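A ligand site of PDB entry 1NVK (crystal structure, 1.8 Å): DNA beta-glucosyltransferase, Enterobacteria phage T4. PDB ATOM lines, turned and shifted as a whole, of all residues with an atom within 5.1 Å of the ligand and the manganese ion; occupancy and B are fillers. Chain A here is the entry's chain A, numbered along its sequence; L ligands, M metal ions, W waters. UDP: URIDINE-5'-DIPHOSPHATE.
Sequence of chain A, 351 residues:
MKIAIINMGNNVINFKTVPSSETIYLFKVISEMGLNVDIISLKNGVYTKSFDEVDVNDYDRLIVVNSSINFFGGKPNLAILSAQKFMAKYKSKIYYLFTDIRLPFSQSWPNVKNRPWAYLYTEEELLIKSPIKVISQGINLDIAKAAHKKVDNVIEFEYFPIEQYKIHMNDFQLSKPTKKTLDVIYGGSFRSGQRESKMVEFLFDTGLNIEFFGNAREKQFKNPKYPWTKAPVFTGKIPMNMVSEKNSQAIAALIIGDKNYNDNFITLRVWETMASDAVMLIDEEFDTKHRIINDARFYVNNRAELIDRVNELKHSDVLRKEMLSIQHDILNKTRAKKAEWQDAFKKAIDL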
ATOM      1  N   VAL A  18      16.869 -32.021  19.165  1.00  0.00           N
ATOM      2  CA  VAL A  18      17.901 -31.000  19.018  1.00  0.00           C
ATOM      3  C   VAL A  18      18.868 -31.183  17.856  1.00  0.00           C
ATOM      4  O   VAL A  18      19.087 -30.252  17.080  1.00  0.00           O
ATOM      5  CB  VAL A  18      18.709 -30.850  20.323  1.00  0.00           C
ATOM      6  CG1 VAL A  18      19.773 -29.760  20.159  1.00  0.00           C
ATOM      7  CG2 VAL A  18      17.777 -30.484  21.474  1.00  0.00           C
ATOM      8  N   THR A  99      31.353 -28.051  16.476  1.00  0.00           N
ATOM      9  CA  THR A  99      30.757 -27.130  17.436  1.00  0.00           C
ATOM     10  C   THR A  99      30.804 -27.601  18.890  1.00  0.00           C
ATOM     11  O   THR A  99      30.514 -26.821  19.799  1.00  0.00           O
ATOM     12  CB  THR A  99      29.269 -26.863  17.091  1.00  0.00           C
ATOM     13  OG1 THR A  99      28.537 -28.091  17.182  1.00  0.00           O
ATOM     14  CG2 THR A  99      29.145 -26.285  15.683  1.00  0.00           C
ATOM     15  N   ASP A 100      31.145 -28.870  19.100  1.00  0.00           N
ATOM     16  CA  ASP A 100      31.221 -29.431  20.457  1.00  0.00           C
ATOM     17  C   ASP A 100      32.555 -30.139  20.601  1.00  0.00           C
ATOM     18  O   ASP A 100      32.849 -31.088  19.874  1.00  0.00           O
ATOM     19  CB  ASP A 100      30.049 -30.391  20.701  1.00  0.00           C
ATOM     20  CG  ASP A 100      29.965 -30.871  22.152  1.00  0.00           C
ATOM     21  OD1 ASP A 100      28.835 -31.129  22.616  1.00  0.00           O
ATOM     22  OD2 ASP A 100      31.006 -31.002  22.814  1.00  0.00           O
ATOM     23  N   GLU A 163      28.060 -21.296  15.309  1.00  0.00           N
ATOM     24  CA  GLU A 163      26.836 -21.099  16.069  1.00  0.00           C
ATOM     25  C   GLU A 163      26.177 -19.720  16.113  1.00  0.00           C
ATOM     26  O   GLU A 163      25.195 -19.517  16.828  1.00  0.00           O
ATOM     27  CB  GLU A 163      27.018 -21.710  17.465  1.00  0.00           C
ATOM     28  CG  GLU A 163      27.101 -23.247  17.349  1.00  0.00           C
ATOM     29  CD  GLU A 163      27.052 -23.985  18.672  1.00  0.00           C
ATOM     30  OE1 GLU A 163      26.471 -25.101  18.683  1.00  0.00           O
ATOM     31  OE2 GLU A 163      27.597 -23.496  19.669  1.00  0.00           O
ATOM     32  N   TYR A 186      18.953 -22.007  33.495  1.00  0.00           N
ATOM     33  CA  TYR A 186      20.015 -22.601  32.679  1.00  0.00           C
ATOM     34  C   TYR A 186      19.453 -23.844  32.003  1.00  0.00           C
ATOM     35  O   TYR A 186      18.866 -24.702  32.661  1.00  0.00           O
ATOM     36  CB  TYR A 186      21.225 -22.974  33.532  1.00  0.00           C
ATOM     37  CG  TYR A 186      22.334 -23.694  32.778  1.00  0.00           C
ATOM     38  CD1 TYR A 186      22.308 -25.085  32.615  1.00  0.00           C
ATOM     39  CD2 TYR A 186      23.398 -22.983  32.212  1.00  0.00           C
ATOM     40  CE1 TYR A 186      23.341 -25.755  31.924  1.00  0.00           C
ATOM     41  CE2 TYR A 186      24.428 -23.636  31.524  1.00  0.00           C
ATOM     42  CZ  TYR A 186      24.393 -25.014  31.376  1.00  0.00           C
ATOM     43  OH  TYR A 186      25.421 -25.647  30.708  1.00  0.00           O
ATOM     44  N   GLY A 187      19.640 -23.946  30.689  1.00  0.00           N
ATOM     45  CA  GLY A 187      19.150 -25.094  29.962  1.00  0.00           C
ATOM     46  C   GLY A 187      20.296 -25.867  29.316  1.00  0.00           C
ATOM     47  O   GLY A 187      21.156 -25.276  28.671  1.00  0.00           O
ATOM     48  N   GLY A 188      20.305 -27.179  29.499  1.00  0.00           N
ATOM     49  CA  GLY A 188      21.362 -27.975  28.909  1.00  0.00           C
ATOM     50  C   GLY A 188      21.369 -29.395  29.435  1.00  0.00           C
ATOM     51  O   GLY A 188      20.492 -29.781  30.194  1.00  0.00           O
ATOM     52  N   SER A 189      22.352 -30.179  28.998  1.00  0.00           N
ATOM     53  CA  SER A 189      22.470 -31.556  29.450  1.00  0.00           C
ATOM     54  C   SER A 189      23.573 -31.638  30.492  1.00  0.00           C
ATOM     55  O   SER A 189      24.247 -30.651  30.781  1.00  0.00           O
ATOM     56  CB  SER A 189      22.824 -32.468  28.277  1.00  0.00           C
ATOM     57  OG  SER A 189      24.186 -32.330  27.925  1.00  0.00           O
ATOM     58  N   ARG A 191      26.269 -33.222  30.124  1.00  0.00           N
ATOM     59  CA  ARG A 191      27.543 -33.266  29.404  1.00  0.00           C
ATOM     60  C   ARG A 191      28.560 -34.210  30.063  1.00  0.00           C
ATOM     61  O   ARG A 191      29.747 -33.915  30.113  1.00  0.00           O
ATOM     62  CB  ARG A 191      28.139 -31.858  29.279  1.00  0.00           C
ATOM     63  CG  ARG A 191      27.301 -30.895  28.426  1.00  0.00           C
ATOM     64  CD  ARG A 191      28.024 -29.571  28.185  1.00  0.00           C
ATOM     65  NE  ARG A 191      29.317 -29.771  27.525  1.00  0.00           N
ATOM     66  CZ  ARG A 191      29.471 -30.083  26.239  1.00  0.00           C
ATOM     67  NH1 ARG A 191      28.398 -30.226  25.459  1.00  0.00           N
ATOM     68  NH2 ARG A 191      30.681 -30.269  25.739  1.00  0.00           N
ATOM     69  N   ARG A 195      31.187 -30.328  33.073  1.00  0.00           N
ATOM     70  CA  ARG A 195      30.965 -28.964  33.535  1.00  0.00           C
ATOM     71  C   ARG A 195      30.341 -28.947  34.937  1.00  0.00           C
ATOM     72  O   ARG A 195      29.803 -27.930  35.380  1.00  0.00           O
ATOM     73  CB  ARG A 195      30.038 -28.276  32.528  1.00  0.00           C
ATOM     74  CG  ARG A 195      29.897 -26.795  32.656  1.00  0.00           C
ATOM     75  CD  ARG A 195      29.001 -26.287  31.523  1.00  0.00           C
ATOM     76  NE  ARG A 195      29.596 -26.554  30.210  1.00  0.00           N
ATOM     77  CZ  ARG A 195      29.006 -26.234  29.053  1.00  0.00           C
ATOM     78  NH1 ARG A 195      27.820 -25.655  29.044  1.00  0.00           N
ATOM     79  NH2 ARG A 195      29.623 -26.482  27.906  1.00  0.00           N
ATOM     80  N   PHE A 213      16.688 -26.572  33.103  1.00  0.00           N
ATOM     81  CA  PHE A 213      15.903 -27.374  32.160  1.00  0.00           C
ATOM     82  C   PHE A 213      16.805 -28.112  31.183  1.00  0.00           C
ATOM     83  O   PHE A 213      17.958 -27.735  30.995  1.00  0.00           O
ATOM     84  CB  PHE A 213      14.849 -26.517  31.405  1.00  0.00           C
ATOM     85  CG  PHE A 213      15.430 -25.470  30.483  1.00  0.00           C
ATOM     86  CD1 PHE A 213      15.881 -24.245  30.985  1.00  0.00           C
ATOM     87  CD2 PHE A 213      15.452 -25.663  29.104  1.00  0.00           C
ATOM     88  CE1 PHE A 213      16.326 -23.238  30.122  1.00  0.00           C
ATOM     89  CE2 PHE A 213      15.901 -24.673  28.238  1.00  0.00           C
ATOM     90  CZ  PHE A 213      16.331 -23.447  28.748  1.00  0.00           C
ATOM     91  N   GLY A 214      16.293 -29.178  30.584  1.00  0.00           N
ATOM     92  CA  GLY A 214      17.100 -29.946  29.659  1.00  0.00           C
ATOM     93  C   GLY A 214      17.158 -31.406  30.069  1.00  0.00           C
ATOM     94  O   GLY A 214      16.390 -31.846  30.922  1.00  0.00           O
ATOM     95  N   GLY A 236      11.955 -30.985  32.465  1.00  0.00           N
ATOM     96  CA  GLY A 236      12.330 -31.680  31.245  1.00  0.00           C
ATOM     97  C   GLY A 236      12.915 -30.828  30.138  1.00  0.00           C
ATOM     98  O   GLY A 236      13.054 -29.618  30.273  1.00  0.00           O
ATOM     99  N   LYS A 237      13.273 -31.470  29.034  1.00  0.00           N
ATOM    100  CA  LYS A 237      13.826 -30.741  27.908  1.00  0.00           C
ATOM    101  C   LYS A 237      12.705 -30.148  27.072  1.00  0.00           C
ATOM    102  O   LYS A 237      11.560 -30.609  27.134  1.00  0.00           O
ATOM    103  CB  LYS A 237      14.703 -31.662  27.054  1.00  0.00           C
ATOM    104  CG  LYS A 237      13.972 -32.838  26.436  1.00  0.00           C
ATOM    105  CD  LYS A 237      14.899 -33.616  25.512  1.00  0.00           C
ATOM    106  CE  LYS A 237      14.166 -34.759  24.840  1.00  0.00           C
ATOM    107  NZ  LYS A 237      15.050 -35.510  23.915  1.00  0.00           N
ATOM    108  N   ILE A 238      13.027 -29.114  26.311  1.00  0.00           N
ATOM    109  CA  ILE A 238      12.063 -28.458  25.445  1.00  0.00           C
ATOM    110  C   ILE A 238      12.666 -28.355  24.050  1.00  0.00           C
ATOM    111  O   ILE A 238      13.887 -28.498  23.872  1.00  0.00           O
ATOM    112  CB  ILE A 238      11.722 -27.041  25.933  1.00  0.00           C
ATOM    113  CG1 ILE A 238      12.989 -26.186  25.996  1.00  0.00           C
ATOM    114  CG2 ILE A 238      11.047 -27.107  27.304  1.00  0.00           C
ATOM    115  CD1 ILE A 238      12.723 -24.711  26.210  1.00  0.00           C
ATOM    116  N   PRO A 239      11.832 -28.093  23.031  1.00  0.00           N
ATOM    117  CA  PRO A 239      12.344 -27.990  21.658  1.00  0.00           C
ATOM    118  C   PRO A 239      13.365 -26.866  21.557  1.00  0.00           C
ATOM    119  O   PRO A 239      13.246 -25.831  22.212  1.00  0.00           O
ATOM    120  CB  PRO A 239      11.079 -27.696  20.850  1.00  0.00           C
ATOM    121  CG  PRO A 239       9.994 -28.356  21.646  1.00  0.00           C
ATOM    122  CD  PRO A 239      10.368 -27.957  23.053  1.00  0.00           C
ATOM    123  N   MET A 240      14.372 -27.066  20.720  1.00  0.00           N
ATOM    124  CA  MET A 240      15.406 -26.066  20.553  1.00  0.00           C
ATOM    125  C   MET A 240      14.843 -24.708  20.141  1.00  0.00           C
ATOM    126  O   MET A 240      15.348 -23.666  20.562  1.00  0.00           O
ATOM    127  CB  MET A 240      16.437 -26.521  19.523  1.00  0.00           C
ATOM    128  CG  MET A 240      17.569 -25.528  19.312  1.00  0.00           C
ATOM    129  SD  MET A 240      18.703 -26.045  18.041  1.00  0.00           S
ATOM    130  CE  MET A 240      19.457 -24.489  17.607  1.00  0.00           C
ATOM    131  N   VAL A 243      13.841 -22.349  23.180  1.00  0.00           N
ATOM    132  CA  VAL A 243      14.824 -22.011  24.208  1.00  0.00           C
ATOM    133  C   VAL A 243      14.885 -20.548  24.656  1.00  0.00           C
ATOM    134  O   VAL A 243      14.906 -20.280  25.861  1.00  0.00           O
ATOM    135  CB  VAL A 243      16.230 -22.476  23.768  1.00  0.00           C
ATOM    136  CG1 VAL A 243      17.290 -22.015  24.769  1.00  0.00           C
ATOM    137  CG2 VAL A 243      16.245 -24.000  23.663  1.00  0.00           C
ATOM    138  N   ILE A 256      28.001 -20.548  31.111  1.00  0.00           N
ATOM    139  CA  ILE A 256      29.183 -21.277  31.566  1.00  0.00           C
ATOM    140  C   ILE A 256      29.564 -22.239  30.436  1.00  0.00           C
ATOM    141  O   ILE A 256      28.778 -22.450  29.508  1.00  0.00           O
ATOM    142  CB  ILE A 256      28.925 -22.129  32.834  1.00  0.00           C
ATOM    143  CG1 ILE A 256      27.675 -22.991  32.628  1.00  0.00           C
ATOM    144  CG2 ILE A 256      28.847 -21.227  34.062  1.00  0.00           C
ATOM    145  CD1 ILE A 256      27.371 -23.940  33.778  1.00  0.00           C
ATOM    146  N   ASP A 258      32.634 -25.666  29.177  1.00  0.00           N
ATOM    147  CA  ASP A 258      33.633 -26.665  29.547  1.00  0.00           C
ATOM    148  C   ASP A 258      34.947 -25.903  29.719  1.00  0.00           C
ATOM    149  O   ASP A 258      35.099 -24.817  29.173  1.00  0.00           O
ATOM    150  CB  ASP A 258      33.795 -27.713  28.434  1.00  0.00           C
ATOM    151  CG  ASP A 258      32.627 -28.691  28.343  1.00  0.00           C
ATOM    152  OD1 ASP A 258      31.544 -28.413  28.912  1.00  0.00           O
ATOM    153  OD2 ASP A 258      32.793 -29.739  27.686  1.00  0.00           O
ATOM    154  N   TYR A 261      36.420 -24.445  26.711  1.00  0.00           N
ATOM    155  CA  TYR A 261      35.595 -23.465  26.013  1.00  0.00           C
ATOM    156  C   TYR A 261      35.964 -22.056  26.462  1.00  0.00           C
ATOM    157  O   TYR A 261      35.739 -21.081  25.742  1.00  0.00           O
ATOM    158  CB  TYR A 261      34.104 -23.677  26.316  1.00  0.00           C
ATOM    159  CG  TYR A 261      33.425 -24.778  25.535  1.00  0.00           C
ATOM    160  CD1 TYR A 261      34.153 -25.625  24.694  1.00  0.00           C
ATOM    161  CD2 TYR A 261      32.049 -24.985  25.641  1.00  0.00           C
ATOM    162  CE1 TYR A 261      33.528 -26.635  23.977  1.00  0.00           C
ATOM    163  CE2 TYR A 261      31.410 -25.998  24.927  1.00  0.00           C
ATOM    164  CZ  TYR A 261      32.158 -26.825  24.097  1.00  0.00           C
ATOM    165  OH  TYR A 261      31.544 -27.826  23.371  1.00  0.00           O
ATOM    166  N   THR A 267      29.584 -20.105  22.433  1.00  0.00           N
ATOM    167  CA  THR A 267      28.529 -21.078  22.175  1.00  0.00           C
ATOM    168  C   THR A 267      27.152 -20.541  21.828  1.00  0.00           C
ATOM    169  O   THR A 267      26.838 -19.373  22.056  1.00  0.00           O
ATOM    170  CB  THR A 267      28.376 -22.030  23.393  1.00  0.00           C
ATOM    171  OG1 THR A 267      28.151 -21.258  24.569  1.00  0.00           O
ATOM    172  CG2 THR A 267      29.650 -22.854  23.579  1.00  0.00           C
ATOM    173  N   LEU A 268      26.321 -21.420  21.272  1.00  0.00           N
ATOM    174  CA  LEU A 268      24.972 -21.060  20.875  1.00  0.00           C
ATOM    175  C   LEU A 268      24.189 -20.445  22.048  1.00  0.00           C
ATOM    176  O   LEU A 268      23.416 -19.515  21.840  1.00  0.00           O
ATOM    177  CB  LEU A 268      24.249 -22.299  20.352  1.00  0.00           C
ATOM    178  CG  LEU A 268      22.774 -22.139  20.015  1.00  0.00           C
ATOM    179  CD1 LEU A 268      22.618 -21.136  18.879  1.00  0.00           C
ATOM    180  CD2 LEU A 268      22.202 -23.494  19.623  1.00  0.00           C
ATOM    181  N   ARG A 269      24.386 -20.960  23.257  1.00  0.00           N
ATOM    182  CA  ARG A 269      23.655 -20.425  24.405  1.00  0.00           C
ATOM    183  C   ARG A 269      23.930 -18.950  24.638  1.00  0.00           C
ATOM    184  O   ARG A 269      23.093 -18.239  25.193  1.00  0.00           O
ATOM    185  CB  ARG A 269      23.932 -21.224  25.688  1.00  0.00           C
ATOM    186  CG  ARG A 269      25.333 -21.086  26.251  1.00  0.00           C
ATOM    187  CD  ARG A 269      25.418 -21.713  27.655  1.00  0.00           C
ATOM    188  NE  ARG A 269      25.141 -23.140  27.626  1.00  0.00           N
ATOM    189  CZ  ARG A 269      23.988 -23.698  27.999  1.00  0.00           C
ATOM    190  NH1 ARG A 269      22.978 -22.950  28.441  1.00  0.00           N
ATOM    191  NH2 ARG A 269      23.837 -25.015  27.911  1.00  0.00           N
ATOM    192  N   GLU A 272      21.393 -17.434  22.390  1.00  0.00           N
ATOM    193  CA  GLU A 272      20.029 -17.735  22.846  1.00  0.00           C
ATOM    194  C   GLU A 272      19.687 -16.943  24.101  1.00  0.00           C
ATOM    195  O   GLU A 272      18.534 -16.586  24.341  1.00  0.00           O
ATOM    196  CB  GLU A 272      19.873 -19.216  23.177  1.00  0.00           C
ATOM    197  CG  GLU A 272      20.080 -20.154  22.007  1.00  0.00           C
ATOM    198  CD  GLU A 272      20.118 -21.612  22.442  1.00  0.00           C
ATOM    199  OE1 GLU A 272      20.661 -21.875  23.528  1.00  0.00           O
ATOM    200  OE2 GLU A 272      19.623 -22.476  21.699  1.00  0.00           O
HETATM  201  N1  UDP L   1      18.743 -27.176  24.452  1.00  0.00           N
HETATM  202  C2  UDP L   1      17.489 -27.384  23.923  1.00  0.00           C
HETATM  203  N3  UDP L   1      16.530 -27.756  24.842  1.00  0.00           N
HETATM  204  C4  UDP L   1      16.694 -27.921  26.197  1.00  0.00           C
HETATM  205  C5  UDP L   1      18.027 -27.650  26.669  1.00  0.00           C
HETATM  206  C6  UDP L   1      18.977 -27.301  25.803  1.00  0.00           C
HETATM  207  O2  UDP L   1      17.236 -27.251  22.744  1.00  0.00           O
HETATM  208  O4  UDP L   1      15.753 -28.328  26.890  1.00  0.00           O
HETATM  209  C1' UDP L   1      19.830 -26.827  23.518  1.00  0.00           C
HETATM  210  C2' UDP L   1      20.040 -25.329  23.327  1.00  0.00           C
HETATM  211  O2' UDP L   1      20.358 -25.055  21.975  1.00  0.00           O
HETATM  212  C3' UDP L   1      21.224 -25.062  24.254  1.00  0.00           C
HETATM  213  C4' UDP L   1      22.041 -26.324  24.086  1.00  0.00           C
HETATM  214  O4' UDP L   1      21.049 -27.376  24.016  1.00  0.00           O
HETATM  215  O3' UDP L   1      21.980 -23.932  23.830  1.00  0.00           O
HETATM  216  C5' UDP L   1      23.025 -26.595  25.209  1.00  0.00           C
HETATM  217  O5' UDP L   1      23.759 -27.798  24.973  1.00  0.00           O
HETATM  218  PA  UDP L   1      24.843 -28.316  26.024  1.00  0.00           P
HETATM  219  O1A UDP L   1      24.117 -28.717  27.255  1.00  0.00           O
HETATM  220  O2A UDP L   1      25.725 -29.296  25.341  1.00  0.00           O
HETATM  221  O3A UDP L   1      25.680 -26.969  26.406  1.00  0.00           O
HETATM  222  PB  UDP L   1      26.808 -26.139  25.583  1.00  0.00           P
HETATM  223  O1B UDP L   1      26.268 -25.974  24.174  1.00  0.00           O
HETATM  224  O2B UDP L   1      28.084 -26.965  25.639  1.00  0.00           O
HETATM  225  O3B UDP L   1      26.938 -24.828  26.333  1.00  0.00           O
HETATM  226 MN    MN M   1      26.986 -26.892  22.210  1.00  0.00          MN
HETATM  227  O   HOH W   1      24.783 -31.842  25.208  1.00  0.00           O
HETATM  228  O   HOH W   2      21.341 -29.935  25.827  1.00  0.00           O
HETATM  229  O   HOH W   3      24.794 -23.810  23.475  1.00  0.00           O
HETATM  230  O   HOH W   4      28.412 -25.459  21.458  1.00  0.00           O
HETATM  231  O   HOH W   5      28.869 -27.839  23.233  1.00  0.00           O
HETATM  232  O   HOH W   6      27.611 -27.933  20.122  1.00  0.00           O
HETATM  233  O   HOH W   7      21.288 -30.604  23.410  1.00  0.00           O
HETATM  234  O   HOH W   8      28.578 -22.818  26.761  1.00  0.00           O
HETATM  235  O   HOH W   9      22.045 -26.903  20.673  1.00  0.00           O
HETATM  236  O   HOH W  10      25.871 -28.718  22.512  1.00  0.00           O
HETATM  237  O   HOH W  11      25.302 -25.890  21.048  1.00  0.00           O
HETATM  238  O   HOH W  12      22.976 -29.284  21.805  1.00  0.00           O
HETATM  239  O   HOH W  13      25.011 -28.205  29.858  1.00  0.00           O
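Water W6 bridges OG1 of Thr 99 (3.1 Å) and OE1 of Glu 163 (3.4 Å).
Water W5 lies within hydrogen-bond range of O2B of the ligand, OH of Tyr 261, NH1 of Arg 191 and OD1 of Asp 100.
Water W8 lies within hydrogen-bond range of O3B of the ligand, OG1 of Thr 267 and O of Ile 256.
Water W3 bridges an oxygen (O3') of the ligand and the backbone NH of Arg 269.
Water W13 lies within hydrogen-bond range of the backbone carbonyl oxygen of Ser 189 (2.7 Å), the side-chain hydroxyl of Tyr 186 (2.7 Å) and an oxygen (O1A) of the ligand (2.8 Å).
Water W2 bridges O4' of the ligand (3.1 Å) and N of Ser 189 (3.3 Å).
The manganese ion is bound by water W4, at 2.2 Å.
Water W10 is bound to the manganese ion (2.2 Å).
Water W11 is bound to the manganese ion (2.3 Å).
O1B of the ligand is bound to the manganese ion, at 2.3 Å.
Water W5 is bound to the manganese ion (2.3 Å).
Water W6 binds the manganese ion (2.4 Å).
The manganese ion has six donor atoms within binding distance.
An oxygen (O3') of the ligand sits at hydrogen-bond distance from the side-chain carboxylate (OE1) of Glu 272 (2.5 Å).
The guanidinium group of Arg 269 is in salt-bridge range of an oxygen (O3B) of the ligand, 2.8 Å away.
The backbone NH of Ser 189 lies within hydrogen-bond range of an oxygen (O1A) of the ligand.
The guanidinium group of Arg 195 is in salt-bridge range of an oxygen (O2B) of the ligand (2.8 Å).
A nitrogen (N3) of the ligand is in hydrogen-bond range of the backbone carbonyl oxygen of Ile 238.
O4 of the ligand sits at hydrogen-bond distance from N of Ile 238 (2.9 Å).
The guanidinium group of Arg 191 is in salt-bridge range of an oxygen (O2A) of the ligand (2.8 Å).
OE1 of Glu 163 touches the manganese ion, at 3.99 Å.
Of the 25 residues printed, 1 comes within 4 Å of the manganese ion.
N of Gly 214 lies within hydrogen-bond range of O of Gly 236, 3.3 Å away.
The guanidinium group (NH2) of Arg 195 is in salt-bridge range of the side-chain carboxylate (OD1) of Asp 258, at 2.9 Å.
The guanidinium group (NH1) of Arg 195 is in hydrogen-bond range of the side-chain hydroxyl (OH) of Tyr 186 (2.9 Å).
The side-chain hydroxyl (OG) of Ser 189 sits close to the backbone NH (N) of Arg 191.
The side-chain hydroxyl (OH) of Tyr 186 is in hydrogen-bond range of the guanidinium group (NH2) of Arg 269 (3.3 Å).
The guanidinium group of Arg 191 lies within salt-bridge range of the side-chain carboxylate of Asp 100 (3.0 Å).
OD2 of Asp 100 sits at hydrogen-bond distance from OH of Tyr 261, 3.3 Å away.
The guanidinium group of Arg 269 is in hydrogen-bond range of the backbone carbonyl oxygen of Gly 187, 2.8 Å away.
Merely in contact with the ligand: Val 18 (3.5 Å), Gly 187 (3.9 Å), Gly 188 (3.3 Å), Phe 213 (3.5 Å), Gly 214 (3.5 Å), Lys 237 (3.3 Å), Met 240 (3.1 Å), Val 243 (3.5 Å), Tyr 261 (3.5 Å) and Leu 268 (3.4 Å).
The nearest printed residue that does not touch the ligand is Pro 239 (4.1 Å).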
